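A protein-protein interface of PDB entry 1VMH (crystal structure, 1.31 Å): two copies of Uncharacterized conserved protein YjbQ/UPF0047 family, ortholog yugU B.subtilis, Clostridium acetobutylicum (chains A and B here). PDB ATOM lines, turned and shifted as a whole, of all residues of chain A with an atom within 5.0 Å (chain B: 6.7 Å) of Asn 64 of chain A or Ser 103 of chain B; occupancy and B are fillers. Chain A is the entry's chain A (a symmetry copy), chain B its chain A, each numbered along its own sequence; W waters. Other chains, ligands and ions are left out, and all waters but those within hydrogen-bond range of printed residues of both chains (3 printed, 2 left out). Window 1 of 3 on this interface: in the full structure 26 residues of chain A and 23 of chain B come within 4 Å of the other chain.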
ATOM      1  N   THR A  62      -4.293   6.382  -9.599  1.00  0.00           N
ATOM      2  CA  THR A  62      -4.471   5.481 -10.722  1.00  0.00           C
ATOM      3  C   THR A  62      -4.910   6.242 -11.953  1.00  0.00           C
ATOM      4  O   THR A  62      -5.216   7.420 -11.865  1.00  0.00           O
ATOM      5  CB  THR A  62      -5.504   4.364 -10.432  1.00  0.00           C
ATOM      6  OG1 THR A  62      -5.319   3.296 -11.399  1.00  0.00           O
ATOM      7  CG2 THR A  62      -6.912   4.877 -10.463  1.00  0.00           C
ATOM      8  N   ILE A  63      -4.915   5.594 -13.103  1.00  0.00           N
ATOM      9  CA  ILE A  63      -5.393   6.229 -14.374  1.00  0.00           C
ATOM     10  C   ILE A  63      -6.459   5.308 -14.902  1.00  0.00           C
ATOM     11  O   ILE A  63      -6.201   4.109 -15.036  1.00  0.00           O
ATOM     12  CB  ILE A  63      -4.227   6.421 -15.353  1.00  0.00           C
ATOM     13  CG1 ILE A  63      -3.194   7.397 -14.748  1.00  0.00           C
ATOM     14  CG2 ILE A  63      -4.693   6.904 -16.709  1.00  0.00           C
ATOM     15  CD1 ILE A  63      -1.971   7.747 -15.589  1.00  0.00           C
ATOM     16  N   ASN A  64      -7.640   5.824 -15.204  1.00  0.00           N
ATOM     17  CA  ASN A  64      -8.703   4.940 -15.639  1.00  0.00           C
ATOM     18  C   ASN A  64      -9.791   5.773 -16.300  1.00  0.00           C
ATOM     19  O   ASN A  64      -9.617   6.966 -16.545  1.00  0.00           O
ATOM     20  CB  ASN A  64      -9.200   4.025 -14.501  1.00  0.00           C
ATOM     21  CG  ASN A  64      -9.616   2.643 -14.993  1.00  0.00           C
ATOM     22  OD1 ASN A  64     -10.510   2.538 -15.832  1.00  0.00           O
ATOM     23  ND2 ASN A  64      -8.952   1.585 -14.497  1.00  0.00           N
ATOM     24  N   GLU A  65     -10.906   5.123 -16.624  1.00  0.00           N
ATOM     25  CA  GLU A  65     -12.065   5.753 -17.269  1.00  0.00           C
ATOM     26  C   GLU A  65     -12.527   6.985 -16.507  1.00  0.00           C
ATOM     27  O   GLU A  65     -12.776   6.898 -15.296  1.00  0.00           O
ATOM     28  CB  GLU A  65     -13.202   4.735 -17.296  1.00  0.00           C
ATOM     29  CG  GLU A  65     -14.590   5.283 -17.596  1.00  0.00           C
ATOM     30  CD  GLU A  65     -14.743   5.702 -19.029  1.00  0.00           C
ATOM     31  OE1 GLU A  65     -14.289   4.962 -19.926  1.00  0.00           O
ATOM     32  OE2 GLU A  65     -15.298   6.786 -19.270  1.00  0.00           O
ATOM     33  N   ASN A  66     -12.718   8.089 -17.233  1.00  0.00           N
ATOM     34  CA  ASN A  66     -13.066   9.347 -16.592  1.00  0.00           C
ATOM     35  C   ASN A  66     -14.381   9.949 -17.015  1.00  0.00           C
ATOM     36  O   ASN A  66     -14.641  11.111 -16.687  1.00  0.00           O
ATOM     37  CB  ASN A  66     -11.928  10.375 -16.854  1.00  0.00           C
ATOM     38  CG  ASN A  66     -11.857  10.791 -18.303  1.00  0.00           C
ATOM     39  OD1 ASN A  66     -12.592  10.261 -19.130  1.00  0.00           O
ATOM     40  ND2 ASN A  66     -11.017  11.809 -18.619  1.00  0.00           N
ATOM     41  N   VAL A  71     -18.117   3.013 -13.700  1.00  0.00           N
ATOM     42  CA  VAL A  71     -16.828   2.326 -13.683  1.00  0.00           C
ATOM     43  C   VAL A  71     -16.118   2.601 -12.385  1.00  0.00           C
ATOM     44  O   VAL A  71     -15.593   1.677 -11.776  1.00  0.00           O
ATOM     45  CB  VAL A  71     -15.947   2.712 -14.867  1.00  0.00           C
ATOM     46  CG1 VAL A  71     -14.506   2.148 -14.696  1.00  0.00           C
ATOM     47  CG2 VAL A  71     -16.567   2.204 -16.143  1.00  0.00           C
ATOM     48  N   ILE A  75     -15.184  -0.214  -9.494  1.00  0.00           N
ATOM     49  CA  ILE A  75     -13.843  -0.458  -8.973  1.00  0.00           C
ATOM     50  C   ILE A  75     -13.826  -0.379  -7.452  1.00  0.00           C
ATOM     51  O   ILE A  75     -13.336  -1.278  -6.783  1.00  0.00           O
ATOM     52  CB  ILE A  75     -12.820   0.533  -9.547  1.00  0.00           C
ATOM     53  CG1 ILE A  75     -12.676   0.350 -11.068  1.00  0.00           C
ATOM     54  CG2 ILE A  75     -11.434   0.339  -8.911  1.00  0.00           C
ATOM     55  CD1 ILE A  75     -11.867   1.433 -11.779  1.00  0.00           C
ATOM     56  N   LEU A 104      -2.167  -1.456  -3.997  1.00  0.00           N
ATOM     57  CA  LEU A 104      -2.652  -2.031  -5.250  1.00  0.00           C
ATOM     58  C   LEU A 104      -2.827  -1.018  -6.354  1.00  0.00           C
ATOM     59  O   LEU A 104      -2.549  -1.311  -7.542  1.00  0.00           O
ATOM     60  CB  LEU A 104      -3.967  -2.782  -5.054  1.00  0.00           C
ATOM     61  CG  LEU A 104      -3.943  -4.053  -4.206  1.00  0.00           C
ATOM     62  CD1 LEU A 104      -5.332  -4.604  -3.888  1.00  0.00           C
ATOM     63  CD2 LEU A 104      -3.117  -5.138  -4.824  1.00  0.00           C
ATOM     64  N   MET A 105      -3.309   0.162  -6.025  1.00  0.00           N
ATOM     65  CA  MET A 105      -3.413   1.239  -7.031  1.00  0.00           C
ATOM     66  C   MET A 105      -2.044   1.794  -7.374  1.00  0.00           C
ATOM     67  O   MET A 105      -1.730   2.056  -8.551  1.00  0.00           O
ATOM     68  CB  MET A 105      -4.326   2.372  -6.530  1.00  0.00           C
ATOM     69  CG  MET A 105      -5.772   1.954  -6.328  1.00  0.00           C
ATOM     70  SD  MET A 105      -6.624   1.427  -7.830  1.00  0.00           S
ATOM     71  CE  MET A 105      -6.386  -0.354  -7.752  1.00  0.00           C
ATOM     72  N   TRP A 123     -11.011   9.072 -23.038  1.00  0.00           N
ATOM     73  CA  TRP A 123     -11.644   9.012 -21.731  1.00  0.00           C
ATOM     74  C   TRP A 123     -10.734   8.390 -20.650  1.00  0.00           C
ATOM     75  O   TRP A 123     -11.203   7.620 -19.818  1.00  0.00           O
ATOM     76  CB  TRP A 123     -13.015   8.275 -21.847  1.00  0.00           C
ATOM     77  CG  TRP A 123     -13.999   8.948 -22.812  1.00  0.00           C
ATOM     78  CD1 TRP A 123     -14.572   8.412 -23.927  1.00  0.00           C
ATOM     79  CD2 TRP A 123     -14.416  10.313 -22.769  1.00  0.00           C
ATOM     80  NE1 TRP A 123     -15.366   9.352 -24.553  1.00  0.00           N
ATOM     81  CE2 TRP A 123     -15.293  10.525 -23.861  1.00  0.00           C
ATOM     82  CE3 TRP A 123     -14.165  11.379 -21.877  1.00  0.00           C
ATOM     83  CZ2 TRP A 123     -15.900  11.760 -24.099  1.00  0.00           C
ATOM     84  CZ3 TRP A 123     -14.786  12.615 -22.121  1.00  0.00           C
ATOM     85  CH2 TRP A 123     -15.636  12.785 -23.221  1.00  0.00           C
ATOM     86  N   GLN A 124      -9.442   8.715 -20.724  1.00  0.00           N
ATOM     87  CA  GLN A 124      -8.488   8.289 -19.771  1.00  0.00           C
ATOM     88  C   GLN A 124      -8.101   9.483 -18.900  1.00  0.00           C
ATOM     89  O   GLN A 124      -7.581  10.466 -19.356  1.00  0.00           O
ATOM     90  CB  GLN A 124      -7.282   7.697 -20.496  1.00  0.00           C
ATOM     91  CG  GLN A 124      -6.321   7.050 -19.581  1.00  0.00           C
ATOM     92  CD  GLN A 124      -5.124   6.462 -20.301  1.00  0.00           C
ATOM     93  OE1 GLN A 124      -4.502   7.105 -21.173  1.00  0.00           O
ATOM     94  NE2 GLN A 124      -4.722   5.269 -19.869  1.00  0.00           N
ATOM     95  N   GLY A 125      -8.345   9.368 -17.595  1.00  0.00           N
ATOM     96  CA  GLY A 125      -8.057  10.426 -16.607  1.00  0.00           C
ATOM     97  C   GLY A 125      -7.238   9.939 -15.455  1.00  0.00           C
ATOM     98  O   GLY A 125      -7.115   8.750 -15.239  1.00  0.00           O
ATOM     99  N   TYR A 127      -6.564   9.896 -11.440  1.00  0.00           N
ATOM    100  CA  TYR A 127      -7.344   9.908 -10.224  1.00  0.00           C
ATOM    101  C   TYR A 127      -6.530   9.773  -8.968  1.00  0.00           C
ATOM    102  O   TYR A 127      -5.629   8.952  -8.879  1.00  0.00           O
ATOM    103  CB  TYR A 127      -8.296   8.734 -10.234  1.00  0.00           C
ATOM    104  CG  TYR A 127      -9.487   8.882 -11.106  1.00  0.00           C
ATOM    105  CD1 TYR A 127     -10.562   9.639 -10.682  1.00  0.00           C
ATOM    106  CD2 TYR A 127      -9.575   8.237 -12.313  1.00  0.00           C
ATOM    107  CE1 TYR A 127     -11.693   9.765 -11.453  1.00  0.00           C
ATOM    108  CE2 TYR A 127     -10.716   8.333 -13.073  1.00  0.00           C
ATOM    109  CZ  TYR A 127     -11.761   9.107 -12.633  1.00  0.00           C
ATOM    110  OH  TYR A 127     -12.934   9.209 -13.386  1.00  0.00           O
ATOM    111  N   THR B  57      -8.000   2.154 -21.051  1.00  0.00           N
ATOM    112  CA  THR B  57      -8.452   1.966 -19.682  1.00  0.00           C
ATOM    113  C   THR B  57      -8.853   0.529 -19.339  1.00  0.00           C
ATOM    114  O   THR B  57      -9.133   0.256 -18.188  1.00  0.00           O
ATOM    115  CB  THR B  57      -9.559   2.924 -19.354  1.00  0.00           C
ATOM    116  OG1 THR B  57     -10.639   2.695 -20.245  1.00  0.00           O
ATOM    117  CG2 THR B  57      -9.075   4.357 -19.463  1.00  0.00           C
ATOM    118  N   THR B  58      -8.840  -0.361 -20.336  1.00  0.00           N
ATOM    119  CA  THR B  58      -9.145  -1.785 -20.150  1.00  0.00           C
ATOM    120  C   THR B  58      -7.950  -2.667 -20.503  1.00  0.00           C
ATOM    121  O   THR B  58      -8.087  -3.866 -20.739  1.00  0.00           O
ATOM    122  CB  THR B  58     -10.357  -2.182 -20.931  1.00  0.00           C
ATOM    123  OG1 THR B  58     -10.174  -1.750 -22.281  1.00  0.00           O
ATOM    124  CG2 THR B  58     -11.600  -1.544 -20.344  1.00  0.00           C
ATOM    125  N   ALA B  59      -6.752  -2.073 -20.454  1.00  0.00           N
ATOM    126  CA  ALA B  59      -5.506  -2.794 -20.593  1.00  0.00           C
ATOM    127  C   ALA B  59      -4.452  -2.071 -19.725  1.00  0.00           C
ATOM    128  O   ALA B  59      -4.684  -0.980 -19.214  1.00  0.00           O
ATOM    129  CB  ALA B  59      -5.090  -2.885 -22.023  1.00  0.00           C
ATOM    130  N   GLY B  60      -3.305  -2.700 -19.562  1.00  0.00           N
ATOM    131  CA  GLY B  60      -2.254  -2.124 -18.757  1.00  0.00           C
ATOM    132  C   GLY B  60      -0.899  -2.655 -19.182  1.00  0.00           C
ATOM    133  O   GLY B  60      -0.748  -3.254 -20.266  1.00  0.00           O
ATOM    134  N   ALA B  98     -12.344  -5.657 -16.533  1.00  0.00           N
ATOM    135  CA  ALA B  98     -11.148  -5.233 -17.279  1.00  0.00           C
ATOM    136  C   ALA B  98     -10.612  -3.914 -16.733  1.00  0.00           C
ATOM    137  O   ALA B  98      -9.395  -3.736 -16.621  1.00  0.00           O
ATOM    138  CB  ALA B  98     -11.444  -5.107 -18.733  1.00  0.00           C
ATOM    139  N   HIS B  99     -11.506  -2.972 -16.433  1.00  0.00           N
ATOM    140  CA  HIS B  99     -11.085  -1.704 -15.845  1.00  0.00           C
ATOM    141  C   HIS B  99     -10.341  -1.934 -14.505  1.00  0.00           C
ATOM    142  O   HIS B  99      -9.326  -1.263 -14.212  1.00  0.00           O
ATOM    143  CB  HIS B  99     -12.276  -0.770 -15.613  1.00  0.00           C
ATOM    144  CG  HIS B  99     -12.841  -0.175 -16.860  1.00  0.00           C
ATOM    145  ND1 HIS B  99     -12.196   0.831 -17.552  1.00  0.00           N
ATOM    146  CD2 HIS B  99     -13.980  -0.430 -17.544  1.00  0.00           C
ATOM    147  CE1 HIS B  99     -12.924   1.162 -18.607  1.00  0.00           C
ATOM    148  NE2 HIS B  99     -14.013   0.421 -18.628  1.00  0.00           N
ATOM    149  N   ILE B 100     -10.843  -2.895 -13.709  1.00  0.00           N
ATOM    150  CA  ILE B 100     -10.238  -3.179 -12.409  1.00  0.00           C
ATOM    151  C   ILE B 100      -8.853  -3.769 -12.612  1.00  0.00           C
ATOM    152  O   ILE B 100      -7.880  -3.338 -12.001  1.00  0.00           O
ATOM    153  CB  ILE B 100     -11.092  -4.151 -11.597  1.00  0.00           C
ATOM    154  CG1 ILE B 100     -12.402  -3.480 -11.171  1.00  0.00           C
ATOM    155  CG2 ILE B 100     -10.347  -4.650 -10.382  1.00  0.00           C
ATOM    156  CD1 ILE B 100     -13.456  -4.464 -10.801  1.00  0.00           C
ATOM    157  N   LYS B 101      -8.774  -4.780 -13.453  1.00  0.00           N
ATOM    158  CA  LYS B 101      -7.505  -5.436 -13.659  1.00  0.00           C
ATOM    159  C   LYS B 101      -6.462  -4.507 -14.275  1.00  0.00           C
ATOM    160  O   LYS B 101      -5.276  -4.582 -13.953  1.00  0.00           O
ATOM    161  CB  LYS B 101      -7.684  -6.711 -14.480  1.00  0.00           C
ATOM    162  CG  LYS B 101      -8.501  -7.743 -13.722  1.00  0.00           C
ATOM    163  CD  LYS B 101      -8.702  -9.079 -14.441  1.00  0.00           C
ATOM    164  CE  LYS B 101      -9.549  -8.991 -15.645  1.00  0.00           C
ATOM    165  NZ  LYS B 101      -9.873 -10.390 -16.249  1.00  0.00           N
ATOM    166  N   ALA B 102      -6.907  -3.643 -15.174  1.00  0.00           N
ATOM    167  CA  ALA B 102      -6.031  -2.639 -15.742  1.00  0.00           C
ATOM    168  C   ALA B 102      -5.397  -1.768 -14.643  1.00  0.00           C
ATOM    169  O   ALA B 102      -4.162  -1.509 -14.664  1.00  0.00           O
ATOM    170  CB  ALA B 102      -6.816  -1.778 -16.747  1.00  0.00           C
ATOM    171  N   SER B 103      -6.185  -1.304 -13.683  1.00  0.00           N
ATOM    172  CA  SER B 103      -5.651  -0.445 -12.604  1.00  0.00           C
ATOM    173  C   SER B 103      -4.706  -1.240 -11.731  1.00  0.00           C
ATOM    174  O   SER B 103      -3.705  -0.705 -11.213  1.00  0.00           O
ATOM    175  CB  SER B 103      -6.758   0.176 -11.749  1.00  0.00           C
ATOM    176  OG  SER B 103      -7.165   1.434 -12.269  1.00  0.00           O
ATOM    177  N   LEU B 104      -5.004  -2.529 -11.546  1.00  0.00           N
ATOM    178  CA  LEU B 104      -4.139  -3.377 -10.728  1.00  0.00           C
ATOM    179  C   LEU B 104      -2.785  -3.633 -11.341  1.00  0.00           C
ATOM    180  O   LEU B 104      -1.758  -3.689 -10.624  1.00  0.00           O
ATOM    181  CB  LEU B 104      -4.801  -4.718 -10.413  1.00  0.00           C
ATOM    182  CG  LEU B 104      -6.039  -4.709  -9.516  1.00  0.00           C
ATOM    183  CD1 LEU B 104      -6.749  -6.058  -9.441  1.00  0.00           C
ATOM    184  CD2 LEU B 104      -5.735  -4.239  -8.127  1.00  0.00           C
ATOM    185  N   MET B 105      -2.733  -3.825 -12.643  1.00  0.00           N
ATOM    186  CA  MET B 105      -1.435  -3.979 -13.330  1.00  0.00           C
ATOM    187  C   MET B 105      -0.701  -2.653 -13.405  1.00  0.00           C
ATOM    188  O   MET B 105       0.524  -2.580 -13.191  1.00  0.00           O
ATOM    189  CB  MET B 105      -1.626  -4.552 -14.745  1.00  0.00           C
ATOM    190  CG  MET B 105      -2.192  -5.960 -14.767  1.00  0.00           C
ATOM    191  SD  MET B 105      -1.140  -7.212 -14.000  1.00  0.00           S
ATOM    192  CE  MET B 105      -1.822  -7.259 -12.336  1.00  0.00           C
ATOM    193  N   GLY B 106      -1.418  -1.589 -13.737  1.00  0.00           N
ATOM    194  CA  GLY B 106      -0.855  -0.289 -13.950  1.00  0.00           C
ATOM    195  C   GLY B 106      -0.949   0.210 -15.376  1.00  0.00           C
ATOM    196  O   GLY B 106      -0.986  -0.556 -16.336  1.00  0.00           O
ATOM    197  N   SER B 107      -0.979   1.540 -15.491  1.00  0.00           N
ATOM    198  CA  SER B 107      -1.058   2.231 -16.774  1.00  0.00           C
ATOM    199  C   SER B 107       0.301   2.399 -17.444  1.00  0.00           C
ATOM    200  O   SER B 107       0.346   2.590 -18.657  1.00  0.00           O
ATOM    201  CB  SER B 107      -1.718   3.607 -16.578  1.00  0.00           C
ATOM    202  OG  SER B 107      -1.017   4.374 -15.585  1.00  0.00           O
ATOM    203  N   PHE B 131      -7.151  -6.868 -21.213  1.00  0.00           N
ATOM    204  CA  PHE B 131      -8.298  -7.428 -20.505  1.00  0.00           C
ATOM    205  C   PHE B 131      -9.675  -7.325 -21.199  1.00  0.00           C
ATOM    206  O   PHE B 131     -10.674  -7.821 -20.649  1.00  0.00           O
ATOM    207  CB  PHE B 131      -8.368  -6.865 -19.094  1.00  0.00           C
ATOM    208  CG  PHE B 131      -7.128  -7.171 -18.283  1.00  0.00           C
ATOM    209  CD1 PHE B 131      -6.807  -8.485 -17.952  1.00  0.00           C
ATOM    210  CD2 PHE B 131      -6.280  -6.148 -17.878  1.00  0.00           C
ATOM    211  CE1 PHE B 131      -5.673  -8.777 -17.197  1.00  0.00           C
ATOM    212  CE2 PHE B 131      -5.134  -6.430 -17.128  1.00  0.00           C
ATOM    213  CZ  PHE B 131      -4.831  -7.722 -16.807  1.00  0.00           C
HETATM  214  O   HOH W   1     -11.988   4.920 -21.115  1.00  0.00           O
HETATM  215  O   HOH W   2      -3.115   1.932 -10.911  1.00  0.00           O
HETATM  216  O   HOH W   3      -2.448   3.323 -13.327  1.00  0.00           O
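Water W1 lies within hydrogen-bond range of the side-chain carboxylate of Glu 65 of chain A (2.6 Å), the side-chain hydroxyl of Thr 57 of chain B (2.7 Å) and the backbone carbonyl oxygen of Trp 123 of chain A (3.1 Å).
Water W2 lies within hydrogen-bond range of OG1 of Thr 62 of chain A (2.6 Å), O of Ser 103 of chain B (2.7 Å) and O of Met 105 of chain A (2.7 Å).
Water W3 lies within hydrogen-bond range of the side-chain hydroxyl (OG) of Ser 107 of chain B (2.9 Å), the backbone NH (N) of Ile 63 of chain A (3.4 Å) and the side-chain hydroxyl (OG1) of Thr 62 of chain A (3.5 Å).
The side-chain amide nitrogen (ND2) of Asn 64 of chain A sits at hydrogen-bond distance from the backbone carbonyl oxygen (O) of His 99 of chain B (2.9 Å).
OG of Ser 103 of chain B sits at hydrogen-bond distance from ND2 of Asn 64 of chain A, 2.9 Å away.
The side-chain hydroxyl (OG) of Ser 103 of chain B is in hydrogen-bond range of the side-chain hydroxyl (OG1) of Thr 62 of chain A, 2.8 Å away.
Of the printed residues of chain B, Thr 62 of chain A touches Ser 103.
Of chain B, only Thr 57 (3.5 Å), His 99 (2.9 Å) and Ser 103 (2.9 Å) come within 4 Å of Asn 64 of chain A.
Of the printed residues of chain B, Trp 123 of chain A touches Thr 57.
Gly 125 of chain A touches none of the printed residues of chain B.
Of the printed residues of chain A, Ile 100 of chain B touches Ile 75 (3.8 Å).
Of the printed residues of chain A, Ser 103 of chain B touches Thr 62 (2.8 Å), Ile 63 (3.97 Å), Asn 64 (2.9 Å) and Leu 104 (3.9 Å).
Printed residues of chain A within 4 Å of Leu 104 of chain B: Leu 104 (3.8 Å) and Met 105 (3.96 Å).
Printed residues of chain A within 4 Å of Ser 107 of chain B: Ile 63 (3.5 Å).
The nearest residue of chain A that does not touch Ser 103 of chain B is Met 105 of chain A (4.05 Å).
O of Trp 123 of chain A is in hydrogen-bond range of N of Asn 66 of chain A (3.0 Å).
The backbone carbonyl oxygen (O) of Thr 62 of chain A is in hydrogen-bond range of the backbone NH (N) of Tyr 127 of chain A, 2.9 Å away.
The side-chain hydroxyl (OH) of Tyr 127 of chain A lies within hydrogen-bond range of the backbone carbonyl oxygen (O) of Glu 65 of chain A (3.0 Å).
A ring nitrogen (ND1) of His 99 of chain B lies within hydrogen-bond range of the backbone carbonyl oxygen of Thr 57 of chain B, at 3.2 Å.
O of Asn 64 of chain A is in hydrogen-bond range of N of Gly 125 of chain A (2.9 Å).
Of the 15 printed residues of chain B, 6 touch a printed residue of chain A.
Hydrophobic or aromatic side chains of chain B within 4 Å of the printed part of chain A: His 99, Ile 100 and Leu 104.
Leu 104 of chain A touches its own counterpart, Leu 104 of chain B.
Met 105 of chain A touches Leu 104 of chain B, but with the chains exchanged Leu 104 of chain A does not touch Met 105 of chain B (5.7 Å).
Positions printed for both chains: 104 and 105.
Of the 15 pairs that touch across the chains among the printed residues, 1 has its exchanged pair printed and touching as well.
Ile 63 of chain A touches Ser 103 of chain B.
Ser 107 of chain B touches Ile 63 of chain A (OG to CD1, 3.5 Å).
Asn 64 of chain A touches Thr 57 of chain B (C to CG2, 3.5 Å).
Glu 65 of chain A touches His 99 of chain B (CB to CE1, 3.8 Å).
Ile 100 of chain B touches Ile 75 of chain A (CG1 to CG1, 3.8 Å).
Ser 103 of chain B touches Leu 104 of chain A.
CB of Leu 104 of chain A touches CD2 of Leu 104 of chain B (3.8 Å).
CD2 of Leu 104 of chain B touches CE of Met 105 of chain A (3.96 Å).
O of Trp 123 of chain A touches CG2 of Thr 57 of chain B, 3.9 Å away.
Gln 124 of chain A touches Thr 57 of chain B (CG to CG2, 3.9 Å).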
